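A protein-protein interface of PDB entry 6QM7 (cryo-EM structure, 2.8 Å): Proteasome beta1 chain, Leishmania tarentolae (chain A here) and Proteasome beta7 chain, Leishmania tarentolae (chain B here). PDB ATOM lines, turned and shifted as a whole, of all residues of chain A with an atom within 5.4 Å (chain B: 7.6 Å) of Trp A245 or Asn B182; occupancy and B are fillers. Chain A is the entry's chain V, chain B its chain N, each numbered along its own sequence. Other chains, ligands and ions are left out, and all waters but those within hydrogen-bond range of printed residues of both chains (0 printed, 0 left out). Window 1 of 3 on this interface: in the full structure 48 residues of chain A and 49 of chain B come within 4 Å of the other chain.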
ATOM      1  N   TYR A 218       5.574  -8.075  15.178  1.00  0.00           N
ATOM      2  CA  TYR A 218       6.264  -9.025  14.277  1.00  0.00           C
ATOM      3  C   TYR A 218       7.740  -8.648  14.198  1.00  0.00           C
ATOM      4  O   TYR A 218       8.542  -9.503  13.759  1.00  0.00           O
ATOM      5  CB  TYR A 218       5.505  -9.241  12.964  1.00  0.00           C
ATOM      6  CG  TYR A 218       5.582  -8.239  11.835  1.00  0.00           C
ATOM      7  CD1 TYR A 218       6.578  -7.287  11.683  1.00  0.00           C
ATOM      8  CD2 TYR A 218       4.652  -8.331  10.824  1.00  0.00           C
ATOM      9  CE1 TYR A 218       6.601  -6.413  10.606  1.00  0.00           C
ATOM     10  CE2 TYR A 218       4.669  -7.483   9.736  1.00  0.00           C
ATOM     11  CZ  TYR A 218       5.639  -6.512   9.625  1.00  0.00           C
ATOM     12  OH  TYR A 218       5.621  -5.693   8.533  1.00  0.00           O
ATOM     13  N   GLY A 226       6.176 -11.019   7.944  1.00  0.00           N
ATOM     14  CA  GLY A 226       5.685 -10.937   6.563  1.00  0.00           C
ATOM     15  C   GLY A 226       4.775  -9.747   6.345  1.00  0.00           C
ATOM     16  O   GLY A 226       5.117  -8.623   6.766  1.00  0.00           O
ATOM     17  N   LEU A 227       3.664  -9.998   5.659  1.00  0.00           N
ATOM     18  CA  LEU A 227       2.675  -8.980   5.252  1.00  0.00           C
ATOM     19  C   LEU A 227       1.835  -8.636   6.475  1.00  0.00           C
ATOM     20  O   LEU A 227       1.592  -9.541   7.289  1.00  0.00           O
ATOM     21  CB  LEU A 227       1.766  -9.555   4.172  1.00  0.00           C
ATOM     22  CG  LEU A 227       2.473 -10.146   2.965  1.00  0.00           C
ATOM     23  CD1 LEU A 227       1.538 -11.076   2.203  1.00  0.00           C
ATOM     24  CD2 LEU A 227       2.993  -9.040   2.073  1.00  0.00           C
ATOM     25  N   ILE A 243      -0.179  -4.614   3.610  1.00  0.00           N
ATOM     26  CA  ILE A 243       1.114  -3.878   3.693  1.00  0.00           C
ATOM     27  C   ILE A 243       2.232  -4.897   3.512  1.00  0.00           C
ATOM     28  O   ILE A 243       2.312  -5.853   4.270  1.00  0.00           O
ATOM     29  CB  ILE A 243       1.260  -3.132   5.034  1.00  0.00           C
ATOM     30  CG1 ILE A 243       0.100  -2.173   5.310  1.00  0.00           C
ATOM     31  CG2 ILE A 243       2.599  -2.423   5.103  1.00  0.00           C
ATOM     32  CD1 ILE A 243       0.086  -0.949   4.423  1.00  0.00           C
ATOM     33  N   PRO A 244       3.102  -4.755   2.494  1.00  0.00           N
ATOM     34  CA  PRO A 244       4.276  -5.610   2.365  1.00  0.00           C
ATOM     35  C   PRO A 244       5.382  -5.192   3.330  1.00  0.00           C
ATOM     36  O   PRO A 244       5.469  -4.025   3.629  1.00  0.00           O
ATOM     37  CB  PRO A 244       4.723  -5.414   0.924  1.00  0.00           C
ATOM     38  CG  PRO A 244       4.256  -4.029   0.600  1.00  0.00           C
ATOM     39  CD  PRO A 244       2.972  -3.826   1.370  1.00  0.00           C
ATOM     40  N   TRP A 245       6.193  -6.151   3.768  1.00  0.00           N
ATOM     41  CA  TRP A 245       7.196  -5.950   4.840  1.00  0.00           C
ATOM     42  C   TRP A 245       8.146  -4.808   4.486  1.00  0.00           C
ATOM     43  O   TRP A 245       8.542  -4.077   5.403  1.00  0.00           O
ATOM     44  CB  TRP A 245       7.964  -7.236   5.131  1.00  0.00           C
ATOM     45  CG  TRP A 245       8.920  -7.032   6.257  1.00  0.00           C
ATOM     46  CD1 TRP A 245       8.686  -7.224   7.586  1.00  0.00           C
ATOM     47  CD2 TRP A 245      10.246  -6.494   6.142  1.00  0.00           C
ATOM     48  NE1 TRP A 245       9.796  -6.867   8.307  1.00  0.00           N
ATOM     49  CE2 TRP A 245      10.759  -6.406   7.446  1.00  0.00           C
ATOM     50  CE3 TRP A 245      11.032  -6.069   5.068  1.00  0.00           C
ATOM     51  CZ2 TRP A 245      12.034  -5.920   7.696  1.00  0.00           C
ATOM     52  CZ3 TRP A 245      12.292  -5.588   5.312  1.00  0.00           C
ATOM     53  CH2 TRP A 245      12.783  -5.513   6.613  1.00  0.00           C
ATOM     54  N   ASN A 246       8.493  -4.654   3.212  1.00  0.00           N
ATOM     55  CA  ASN A 246       9.405  -3.585   2.729  1.00  0.00           C
ATOM     56  C   ASN A 246       8.769  -2.191   2.875  1.00  0.00           C
ATOM     57  O   ASN A 246       9.508  -1.211   2.714  1.00  0.00           O
ATOM     58  CB  ASN A 246       9.860  -3.868   1.298  1.00  0.00           C
ATOM     59  CG  ASN A 246       8.731  -3.823   0.303  1.00  0.00           C
ATOM     60  OD1 ASN A 246       8.350  -2.746  -0.151  1.00  0.00           O
ATOM     61  ND2 ASN A 246       8.209  -4.987  -0.050  1.00  0.00           N
ATOM     62  N   ARG A 247       7.465  -2.087   3.147  1.00  0.00           N
ATOM     63  CA  ARG A 247       6.763  -0.800   3.392  1.00  0.00           C
ATOM     64  C   ARG A 247       6.121  -0.803   4.782  1.00  0.00           C
ATOM     65  O   ARG A 247       5.196   0.007   5.002  1.00  0.00           O
ATOM     66  CB  ARG A 247       5.712  -0.561   2.303  1.00  0.00           C
ATOM     67  CG  ARG A 247       6.260   0.110   1.054  1.00  0.00           C
ATOM     68  CD  ARG A 247       5.161   0.733   0.208  1.00  0.00           C
ATOM     69  NE  ARG A 247       4.437  -0.272  -0.575  1.00  0.00           N
ATOM     70  CZ  ARG A 247       3.192  -0.727  -0.361  1.00  0.00           C
ATOM     71  NH1 ARG A 247       2.699  -1.643  -1.183  1.00  0.00           N
ATOM     72  NH2 ARG A 247       2.441  -0.286   0.641  1.00  0.00           N
ATOM     73  N   SER A 248       6.576  -1.651   5.705  1.00  0.00           N
ATOM     74  CA  SER A 248       5.936  -1.761   7.037  1.00  0.00           C
ATOM     75  C   SER A 248       6.137  -0.453   7.786  1.00  0.00           C
ATOM     76  O   SER A 248       7.158   0.210   7.603  1.00  0.00           O
ATOM     77  CB  SER A 248       6.397  -2.960   7.839  1.00  0.00           C
ATOM     78  OG  SER A 248       7.729  -2.826   8.294  1.00  0.00           O
ATOM     79  N   CYS A 251       9.920  -1.392  11.606  1.00  0.00           N
ATOM     80  CA  CYS A 251      10.793  -2.573  11.792  1.00  0.00           C
ATOM     81  C   CYS A 251      12.063  -2.095  12.496  1.00  0.00           C
ATOM     82  O   CYS A 251      12.414  -0.903  12.339  1.00  0.00           O
ATOM     83  CB  CYS A 251      11.076  -3.254  10.458  1.00  0.00           C
ATOM     84  SG  CYS A 251      12.105  -2.267   9.334  1.00  0.00           S
ATOM     85  N   GLU A 253      15.052  -2.954  11.903  1.00  0.00           N
ATOM     86  CA  GLU A 253      16.154  -2.890  10.920  1.00  0.00           C
ATOM     87  C   GLU A 253      16.310  -1.455  10.411  1.00  0.00           C
ATOM     88  O   GLU A 253      17.442  -1.079  10.088  1.00  0.00           O
ATOM     89  CB  GLU A 253      15.874  -3.877   9.787  1.00  0.00           C
ATOM     90  CG  GLU A 253      15.828  -5.337  10.233  1.00  0.00           C
ATOM     91  CD  GLU A 253      14.455  -5.959  10.478  1.00  0.00           C
ATOM     92  OE1 GLU A 253      13.668  -5.382  11.263  1.00  0.00           O
ATOM     93  OE2 GLU A 253      14.178  -7.045   9.907  1.00  0.00           O
ATOM     94  N   LYS A 254      15.213  -0.699  10.359  1.00  0.00           N
ATOM     95  CA  LYS A 254      15.142   0.674   9.797  1.00  0.00           C
ATOM     96  C   LYS A 254      15.059   1.723  10.916  1.00  0.00           C
ATOM     97  O   LYS A 254      15.264   2.907  10.609  1.00  0.00           O
ATOM     98  CB  LYS A 254      13.957   0.745   8.827  1.00  0.00           C
ATOM     99  CG  LYS A 254      14.151  -0.072   7.552  1.00  0.00           C
ATOM    100  CD  LYS A 254      13.167   0.254   6.444  1.00  0.00           C
ATOM    101  CE  LYS A 254      13.400  -0.535   5.169  1.00  0.00           C
ATOM    102  NZ  LYS A 254      12.729  -1.859   5.211  1.00  0.00           N
ATOM    103  N   ASP B  21      23.108 -12.381   9.773  1.00  0.00           N
ATOM    104  CA  ASP B  21      22.174 -11.400  10.382  1.00  0.00           C
ATOM    105  C   ASP B  21      22.843 -10.827  11.633  1.00  0.00           C
ATOM    106  O   ASP B  21      23.690 -11.506  12.228  1.00  0.00           O
ATOM    107  CB  ASP B  21      20.771 -11.978  10.652  1.00  0.00           C
ATOM    108  CG  ASP B  21      20.587 -13.002  11.787  1.00  0.00           C
ATOM    109  OD1 ASP B  21      21.380 -12.994  12.756  1.00  0.00           O
ATOM    110  OD2 ASP B  21      19.623 -13.817  11.701  1.00  0.00           O
ATOM    111  N   THR B  22      22.494  -9.599  11.991  1.00  0.00           N
ATOM    112  CA  THR B  22      23.034  -8.918  13.180  1.00  0.00           C
ATOM    113  C   THR B  22      21.994  -9.046  14.268  1.00  0.00           C
ATOM    114  O   THR B  22      21.563  -8.016  14.776  1.00  0.00           O
ATOM    115  CB  THR B  22      23.395  -7.467  12.864  1.00  0.00           C
ATOM    116  OG1 THR B  22      22.223  -6.676  12.647  1.00  0.00           O
ATOM    117  CG2 THR B  22      24.313  -7.392  11.667  1.00  0.00           C
ATOM    118  N   LEU B  23      21.580 -10.267  14.569  1.00  0.00           N
ATOM    119  CA  LEU B  23      20.465 -10.496  15.511  1.00  0.00           C
ATOM    120  C   LEU B  23      20.803 -11.652  16.417  1.00  0.00           C
ATOM    121  O   LEU B  23      21.095 -12.734  15.899  1.00  0.00           O
ATOM    122  CB  LEU B  23      19.172 -10.795  14.755  1.00  0.00           C
ATOM    123  CG  LEU B  23      18.018 -11.328  15.609  1.00  0.00           C
ATOM    124  CD1 LEU B  23      17.272 -10.202  16.294  1.00  0.00           C
ATOM    125  CD2 LEU B  23      17.067 -12.159  14.779  1.00  0.00           C
ATOM    126  N   LEU B 170      20.799 -14.577   1.561  1.00  0.00           N
ATOM    127  CA  LEU B 170      20.368 -13.768   2.731  1.00  0.00           C
ATOM    128  C   LEU B 170      18.892 -13.410   2.545  1.00  0.00           C
ATOM    129  O   LEU B 170      18.116 -13.561   3.505  1.00  0.00           O
ATOM    130  CB  LEU B 170      21.239 -12.510   2.846  1.00  0.00           C
ATOM    131  CG  LEU B 170      22.721 -12.771   3.121  1.00  0.00           C
ATOM    132  CD1 LEU B 170      23.514 -11.471   3.248  1.00  0.00           C
ATOM    133  CD2 LEU B 170      22.898 -13.650   4.354  1.00  0.00           C
ATOM    134  N   ARG B 171      18.522 -12.978   1.344  1.00  0.00           N
ATOM    135  CA  ARG B 171      17.116 -12.663   0.996  1.00  0.00           C
ATOM    136  C   ARG B 171      16.240 -13.853   1.362  1.00  0.00           C
ATOM    137  O   ARG B 171      15.232 -13.644   2.021  1.00  0.00           O
ATOM    138  CB  ARG B 171      16.963 -12.338  -0.485  1.00  0.00           C
ATOM    139  CG  ARG B 171      15.797 -11.414  -0.786  1.00  0.00           C
ATOM    140  CD  ARG B 171      15.571 -11.251  -2.286  1.00  0.00           C
ATOM    141  NE  ARG B 171      16.792 -11.276  -3.085  1.00  0.00           N
ATOM    142  CZ  ARG B 171      17.675 -10.285  -3.191  1.00  0.00           C
ATOM    143  NH1 ARG B 171      18.746 -10.438  -3.951  1.00  0.00           N
ATOM    144  NH2 ARG B 171      17.500  -9.146  -2.548  1.00  0.00           N
ATOM    145  N   PHE B 174      16.002 -14.528   5.057  1.00  0.00           N
ATOM    146  CA  PHE B 174      15.102 -13.517   5.636  1.00  0.00           C
ATOM    147  C   PHE B 174      13.655 -13.961   5.459  1.00  0.00           C
ATOM    148  O   PHE B 174      12.898 -13.843   6.420  1.00  0.00           O
ATOM    149  CB  PHE B 174      15.319 -12.141   5.024  1.00  0.00           C
ATOM    150  CG  PHE B 174      14.319 -11.175   5.579  1.00  0.00           C
ATOM    151  CD1 PHE B 174      14.266 -10.947   6.947  1.00  0.00           C
ATOM    152  CD2 PHE B 174      13.378 -10.580   4.753  1.00  0.00           C
ATOM    153  CE1 PHE B 174      13.318 -10.096   7.479  1.00  0.00           C
ATOM    154  CE2 PHE B 174      12.436  -9.715   5.283  1.00  0.00           C
ATOM    155  CZ  PHE B 174      12.416  -9.475   6.643  1.00  0.00           C
ATOM    156  N   TYR B 175      13.292 -14.472   4.285  1.00  0.00           N
ATOM    157  CA  TYR B 175      11.914 -14.925   3.973  1.00  0.00           C
ATOM    158  C   TYR B 175      11.523 -16.150   4.801  1.00  0.00           C
ATOM    159  O   TYR B 175      10.338 -16.237   5.176  1.00  0.00           O
ATOM    160  CB  TYR B 175      11.770 -15.330   2.516  1.00  0.00           C
ATOM    161  CG  TYR B 175      11.914 -14.247   1.480  1.00  0.00           C
ATOM    162  CD1 TYR B 175      11.440 -12.960   1.659  1.00  0.00           C
ATOM    163  CD2 TYR B 175      12.499 -14.548   0.265  1.00  0.00           C
ATOM    164  CE1 TYR B 175      11.545 -12.006   0.653  1.00  0.00           C
ATOM    165  CE2 TYR B 175      12.622 -13.610  -0.742  1.00  0.00           C
ATOM    166  CZ  TYR B 175      12.118 -12.339  -0.563  1.00  0.00           C
ATOM    167  OH  TYR B 175      12.267 -11.462  -1.599  1.00  0.00           O
ATOM    168  N   ALA B 180      15.186 -14.319  12.157  1.00  0.00           N
ATOM    169  CA  ALA B 180      16.088 -13.524  11.312  1.00  0.00           C
ATOM    170  C   ALA B 180      15.601 -12.078  11.292  1.00  0.00           C
ATOM    171  O   ALA B 180      14.435 -11.810  11.641  1.00  0.00           O
ATOM    172  CB  ALA B 180      16.141 -14.111   9.928  1.00  0.00           C
ATOM    173  N   ILE B 181      16.509 -11.185  10.938  1.00  0.00           N
ATOM    174  CA  ILE B 181      16.196  -9.792  10.555  1.00  0.00           C
ATOM    175  C   ILE B 181      16.820  -9.579   9.183  1.00  0.00           C
ATOM    176  O   ILE B 181      17.689 -10.371   8.796  1.00  0.00           O
ATOM    177  CB  ILE B 181      16.727  -8.775  11.579  1.00  0.00           C
ATOM    178  CG1 ILE B 181      18.232  -8.926  11.818  1.00  0.00           C
ATOM    179  CG2 ILE B 181      15.950  -8.823  12.878  1.00  0.00           C
ATOM    180  CD1 ILE B 181      18.815  -7.784  12.609  1.00  0.00           C
ATOM    181  N   ASN B 182      16.358  -8.538   8.505  1.00  0.00           N
ATOM    182  CA  ASN B 182      16.901  -8.037   7.229  1.00  0.00           C
ATOM    183  C   ASN B 182      17.954  -6.995   7.597  1.00  0.00           C
ATOM    184  O   ASN B 182      17.773  -5.810   7.266  1.00  0.00           O
ATOM    185  CB  ASN B 182      15.764  -7.522   6.346  1.00  0.00           C
ATOM    186  CG  ASN B 182      16.209  -7.205   4.939  1.00  0.00           C
ATOM    187  OD1 ASN B 182      17.401  -7.197   4.644  1.00  0.00           O
ATOM    188  ND2 ASN B 182      15.251  -6.953   4.065  1.00  0.00           N
ATOM    189  N   LYS B 183      18.976  -7.419   8.330  1.00  0.00           N
ATOM    190  CA  LYS B 183      20.206  -6.621   8.528  1.00  0.00           C
ATOM    191  C   LYS B 183      21.353  -7.598   8.672  1.00  0.00           C
ATOM    192  O   LYS B 183      21.311  -8.410   9.595  1.00  0.00           O
ATOM    193  CB  LYS B 183      20.134  -5.672   9.728  1.00  0.00           C
ATOM    194  CG  LYS B 183      20.852  -4.344   9.503  1.00  0.00           C
ATOM    195  CD  LYS B 183      20.353  -3.228  10.398  1.00  0.00           C
ATOM    196  CE  LYS B 183      20.808  -3.407  11.840  1.00  0.00           C
ATOM    197  NZ  LYS B 183      19.748  -3.052  12.818  1.00  0.00           N
ATOM    198  N   PHE B 184      22.321  -7.503   7.774  1.00  0.00           N
ATOM    199  CA  PHE B 184      23.435  -8.462   7.640  1.00  0.00           C
ATOM    200  C   PHE B 184      24.754  -7.732   7.728  1.00  0.00           C
ATOM    201  O   PHE B 184      24.784  -6.525   7.613  1.00  0.00           O
ATOM    202  CB  PHE B 184      23.306  -9.178   6.305  1.00  0.00           C
ATOM    203  CG  PHE B 184      21.953  -9.811   6.139  1.00  0.00           C
ATOM    204  CD1 PHE B 184      21.668 -11.021   6.749  1.00  0.00           C
ATOM    205  CD2 PHE B 184      20.961  -9.178   5.411  1.00  0.00           C
ATOM    206  CE1 PHE B 184      20.419 -11.602   6.605  1.00  0.00           C
ATOM    207  CE2 PHE B 184      19.717  -9.769   5.252  1.00  0.00           C
ATOM    208  CZ  PHE B 184      19.441 -10.972   5.862  1.00  0.00           C
ATOM    209  N   PRO B 199      26.634  -2.815   8.384  1.00  0.00           N
ATOM    210  CA  PRO B 199      25.427  -3.619   8.208  1.00  0.00           C
ATOM    211  C   PRO B 199      24.580  -3.136   7.023  1.00  0.00           C
ATOM    212  O   PRO B 199      24.493  -1.949   6.815  1.00  0.00           O
ATOM    213  CB  PRO B 199      24.663  -3.456   9.526  1.00  0.00           C
ATOM    214  CG  PRO B 199      25.714  -3.010  10.509  1.00  0.00           C
ATOM    215  CD  PRO B 199      26.696  -2.184   9.706  1.00  0.00           C
ATOM    216  N   PHE B 200      24.013  -4.058   6.260  1.00  0.00           N
ATOM    217  CA  PHE B 200      23.133  -3.733   5.114  1.00  0.00           C
ATOM    218  C   PHE B 200      21.844  -4.550   5.201  1.00  0.00           C
ATOM    219  O   PHE B 200      21.813  -5.556   5.916  1.00  0.00           O
ATOM    220  CB  PHE B 200      23.871  -3.961   3.794  1.00  0.00           C
ATOM    221  CG  PHE B 200      24.261  -5.391   3.537  1.00  0.00           C
ATOM    222  CD1 PHE B 200      23.445  -6.234   2.795  1.00  0.00           C
ATOM    223  CD2 PHE B 200      25.442  -5.898   4.048  1.00  0.00           C
ATOM    224  CE1 PHE B 200      23.803  -7.557   2.578  1.00  0.00           C
ATOM    225  CE2 PHE B 200      25.800  -7.219   3.825  1.00  0.00           C
ATOM    226  CZ  PHE B 200      24.984  -8.046   3.089  1.00  0.00           C
ATOM    227  N   ASP B 201      20.819  -4.107   4.476  1.00  0.00           N
ATOM    228  CA  ASP B 201      19.571  -4.869   4.216  1.00  0.00           C
ATOM    229  C   ASP B 201      19.599  -5.350   2.766  1.00  0.00           C
ATOM    230  O   ASP B 201      20.479  -4.920   2.015  1.00  0.00           O
ATOM    231  CB  ASP B 201      18.325  -4.037   4.539  1.00  0.00           C
ATOM    232  CG  ASP B 201      18.091  -2.831   3.636  1.00  0.00           C
ATOM    233  OD1 ASP B 201      19.015  -2.475   2.866  1.00  0.00           O
ATOM    234  OD2 ASP B 201      16.983  -2.239   3.714  1.00  0.00           O
ATOM    235  N   VAL B 202      18.666  -6.221   2.407  1.00  0.00           N
ATOM    236  CA  VAL B 202      18.482  -6.749   1.027  1.00  0.00           C
ATOM    237  C   VAL B 202      17.060  -6.387   0.586  1.00  0.00           C
ATOM    238  O   VAL B 202      16.154  -6.406   1.437  1.00  0.00           O
ATOM    239  CB  VAL B 202      18.769  -8.263   0.970  1.00  0.00           C
ATOM    240  CG1 VAL B 202      20.142  -8.592   1.523  1.00  0.00           C
ATOM    241  CG2 VAL B 202      17.730  -9.087   1.696  1.00  0.00           C
ATOM    242  N   GLU B 203      16.878  -6.011  -0.681  1.00  0.00           N
ATOM    243  CA  GLU B 203      15.532  -5.739  -1.251  1.00  0.00           C
ATOM    244  C   GLU B 203      14.725  -7.028  -1.146  1.00  0.00           C
ATOM    245  O   GLU B 203      15.301  -8.088  -1.381  1.00  0.00           O
ATOM    246  CB  GLU B 203      15.622  -5.250  -2.696  1.00  0.00           C
ATOM    247  CG  GLU B 203      15.813  -3.745  -2.820  1.00  0.00           C
ATOM    248  CD  GLU B 203      16.348  -3.293  -4.175  1.00  0.00           C
ATOM    249  OE1 GLU B 203      17.589  -3.226  -4.330  1.00  0.00           O
ATOM    250  OE2 GLU B 203      15.525  -3.029  -5.085  1.00  0.00           O
ATOM    251  N   THR B 204      13.451  -6.935  -0.783  1.00  0.00           N
ATOM    252  CA  THR B 204      12.566  -8.105  -0.548  1.00  0.00           C
ATOM    253  C   THR B 204      11.265  -7.923  -1.331  1.00  0.00           C
ATOM    254  O   THR B 204      10.653  -6.862  -1.215  1.00  0.00           O
ATOM    255  CB  THR B 204      12.341  -8.307   0.954  1.00  0.00           C
ATOM    256  OG1 THR B 204      12.091  -7.054   1.596  1.00  0.00           O
ATOM    257  CG2 THR B 204      13.518  -8.976   1.633  1.00  0.00           C
ATOM    258  N   HIS B 205      10.882  -8.917  -2.122  1.00  0.00           N
ATOM    259  CA  HIS B 205       9.637  -8.900  -2.922  1.00  0.00           C
ATOM    260  C   HIS B 205       8.533  -9.567  -2.095  1.00  0.00           C
ATOM    261  O   HIS B 205       8.755 -10.671  -1.577  1.00  0.00           O
ATOM    262  CB  HIS B 205       9.871  -9.495  -4.320  1.00  0.00           C
ATOM    263  CG  HIS B 205       8.759  -9.189  -5.275  1.00  0.00           C
ATOM    264  ND1 HIS B 205       8.011  -8.019  -5.199  1.00  0.00           N
ATOM    265  CD2 HIS B 205       8.260  -9.882  -6.325  1.00  0.00           C
ATOM    266  CE1 HIS B 205       7.099  -8.014  -6.153  1.00  0.00           C
ATOM    267  NE2 HIS B 205       7.230  -9.148  -6.862  1.00  0.00           N
ATOM    268  N   TRP B 206       7.413  -8.860  -1.933  1.00  0.00           N
ATOM    269  CA  TRP B 206       6.231  -9.260  -1.128  1.00  0.00           C
ATOM    270  C   TRP B 206       4.930  -9.112  -1.926  1.00  0.00           C
ATOM    271  O   TRP B 206       3.875  -9.476  -1.379  1.00  0.00           O
ATOM    272  CB  TRP B 206       6.193  -8.386   0.123  1.00  0.00           C
ATOM    273  CG  TRP B 206       7.299  -8.711   1.065  1.00  0.00           C
ATOM    274  CD1 TRP B 206       8.523  -8.116   1.193  1.00  0.00           C
ATOM    275  CD2 TRP B 206       7.267  -9.780   2.005  1.00  0.00           C
ATOM    276  NE1 TRP B 206       9.253  -8.745   2.166  1.00  0.00           N
ATOM    277  CE2 TRP B 206       8.511  -9.778   2.665  1.00  0.00           C
ATOM    278  CE3 TRP B 206       6.300 -10.738   2.337  1.00  0.00           C
ATOM    279  CZ2 TRP B 206       8.806 -10.708   3.656  1.00  0.00           C
ATOM    280  CZ3 TRP B 206       6.589 -11.648   3.321  1.00  0.00           C
ATOM    281  CH2 TRP B 206       7.831 -11.638   3.960  1.00  0.00           C
ATOM    282  N   GLU B 207       4.997  -8.593  -3.153  1.00  0.00           N
ATOM    283  CA  GLU B 207       3.817  -8.143  -3.928  1.00  0.00           C
ATOM    284  C   GLU B 207       3.662  -9.046  -5.152  1.00  0.00           C
ATOM    285  O   GLU B 207       3.409  -8.518  -6.256  1.00  0.00           O
ATOM    286  CB  GLU B 207       3.969  -6.660  -4.274  1.00  0.00           C
ATOM    287  CG  GLU B 207       3.620  -5.731  -3.119  1.00  0.00           C
ATOM    288  CD  GLU B 207       4.458  -4.462  -3.056  1.00  0.00           C
ATOM    289  OE1 GLU B 207       5.646  -4.555  -2.642  1.00  0.00           O
ATOM    290  OE2 GLU B 207       3.928  -3.381  -3.417  1.00  0.00           O
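O of Trp A245 lies within hydrogen-bond range of OG of Ser A248 (3.3 Å). The backbone NH (N) of Val B202 sits at hydrogen-bond distance from the side-chain amide oxygen (OD1) of Asn B182, at 2.7 Å. The side-chain hydroxyl (OH) of Tyr A218 sits close to the backbone carbonyl oxygen (O) of Gly A226. O of Lys B183 sits at hydrogen-bond distance from N of Thr B22, 2.9 Å away. The side-chain hydroxyl (OG1) of Thr B204 sits close to the indole nitrogen (NE1) of Trp B206 (3.4 Å).
Trp A245 touches just these residues of chain B: Phe B174, Asn B182, Thr B204 and Trp B206. Printed residues of chain A within 4 Å of Asn B182: Trp A245 (3.5 Å) and Glu A253 (3.0 Å). Of the printed residues of chain A, Thr B204 touches Trp A245 (3.8 Å) and Asn A246 (3.3 Å). Of the printed residues of chain B, Asn A246 touches Thr B204, Trp B206 and Glu B207. Tyr B175 touches none of the printed residues of chain A. The nearest residue of chain B that does not touch Trp A245 is Val B202 (5.5 Å). The nearest printed residue of chain A that does not touch Asn B182 is Lys A254 (5.8 Å).
The side-chain amide nitrogen (ND2) of Asn A246 lies within hydrogen-bond range of the backbone carbonyl oxygen (O) of Thr B204 (3.3 Å). The side-chain carboxylate (OE2) of Glu A253 is in hydrogen-bond range of the backbone NH (N) of Asn B182 (3.0 Å). The side-chain carboxylate of Glu B207 is in salt-bridge range of the guanidinium group of Arg A247 (3.1 Å).
Hydrophobic or aromatic side chains of chain A within 4 Å of the printed part of chain B: Leu A227, Pro A244 and Trp A245. Of the 21 printed residues of chain B, 7 touch a printed residue of chain A. Printed residues of chain B that touch a printed residue of chain A: Phe B174, Ile B181, Asn B182, Lys B183, Thr B204, Trp B206 and Glu B207. Among the printed residues, 16 pairs touch across the chains.
Among the printed residues, merely in contact across the chains: Gly A226 with Trp B206 (3.4 Å), Leu A227 with Trp B206 (3.6 Å), Pro A244 with Trp B206 (3.4 Å), Pro A244 with Glu B207 (3.6 Å), Trp A245 with Phe B174 (3.6 Å), Trp A245 with Asn B182 (3.5 Å), Trp A245 with Thr B204 (3.8 Å), Trp A245 with Trp B206 (3.6 Å), Asn A246 with Trp B206 (3.4 Å), Asn A246 with Glu B207 (3.7 Å), Glu A253 with Phe B174 (3.99 Å), Glu A253 with Ile B181 (3.5 Å) and Glu A253 with Lys B183 (3.6 Å).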
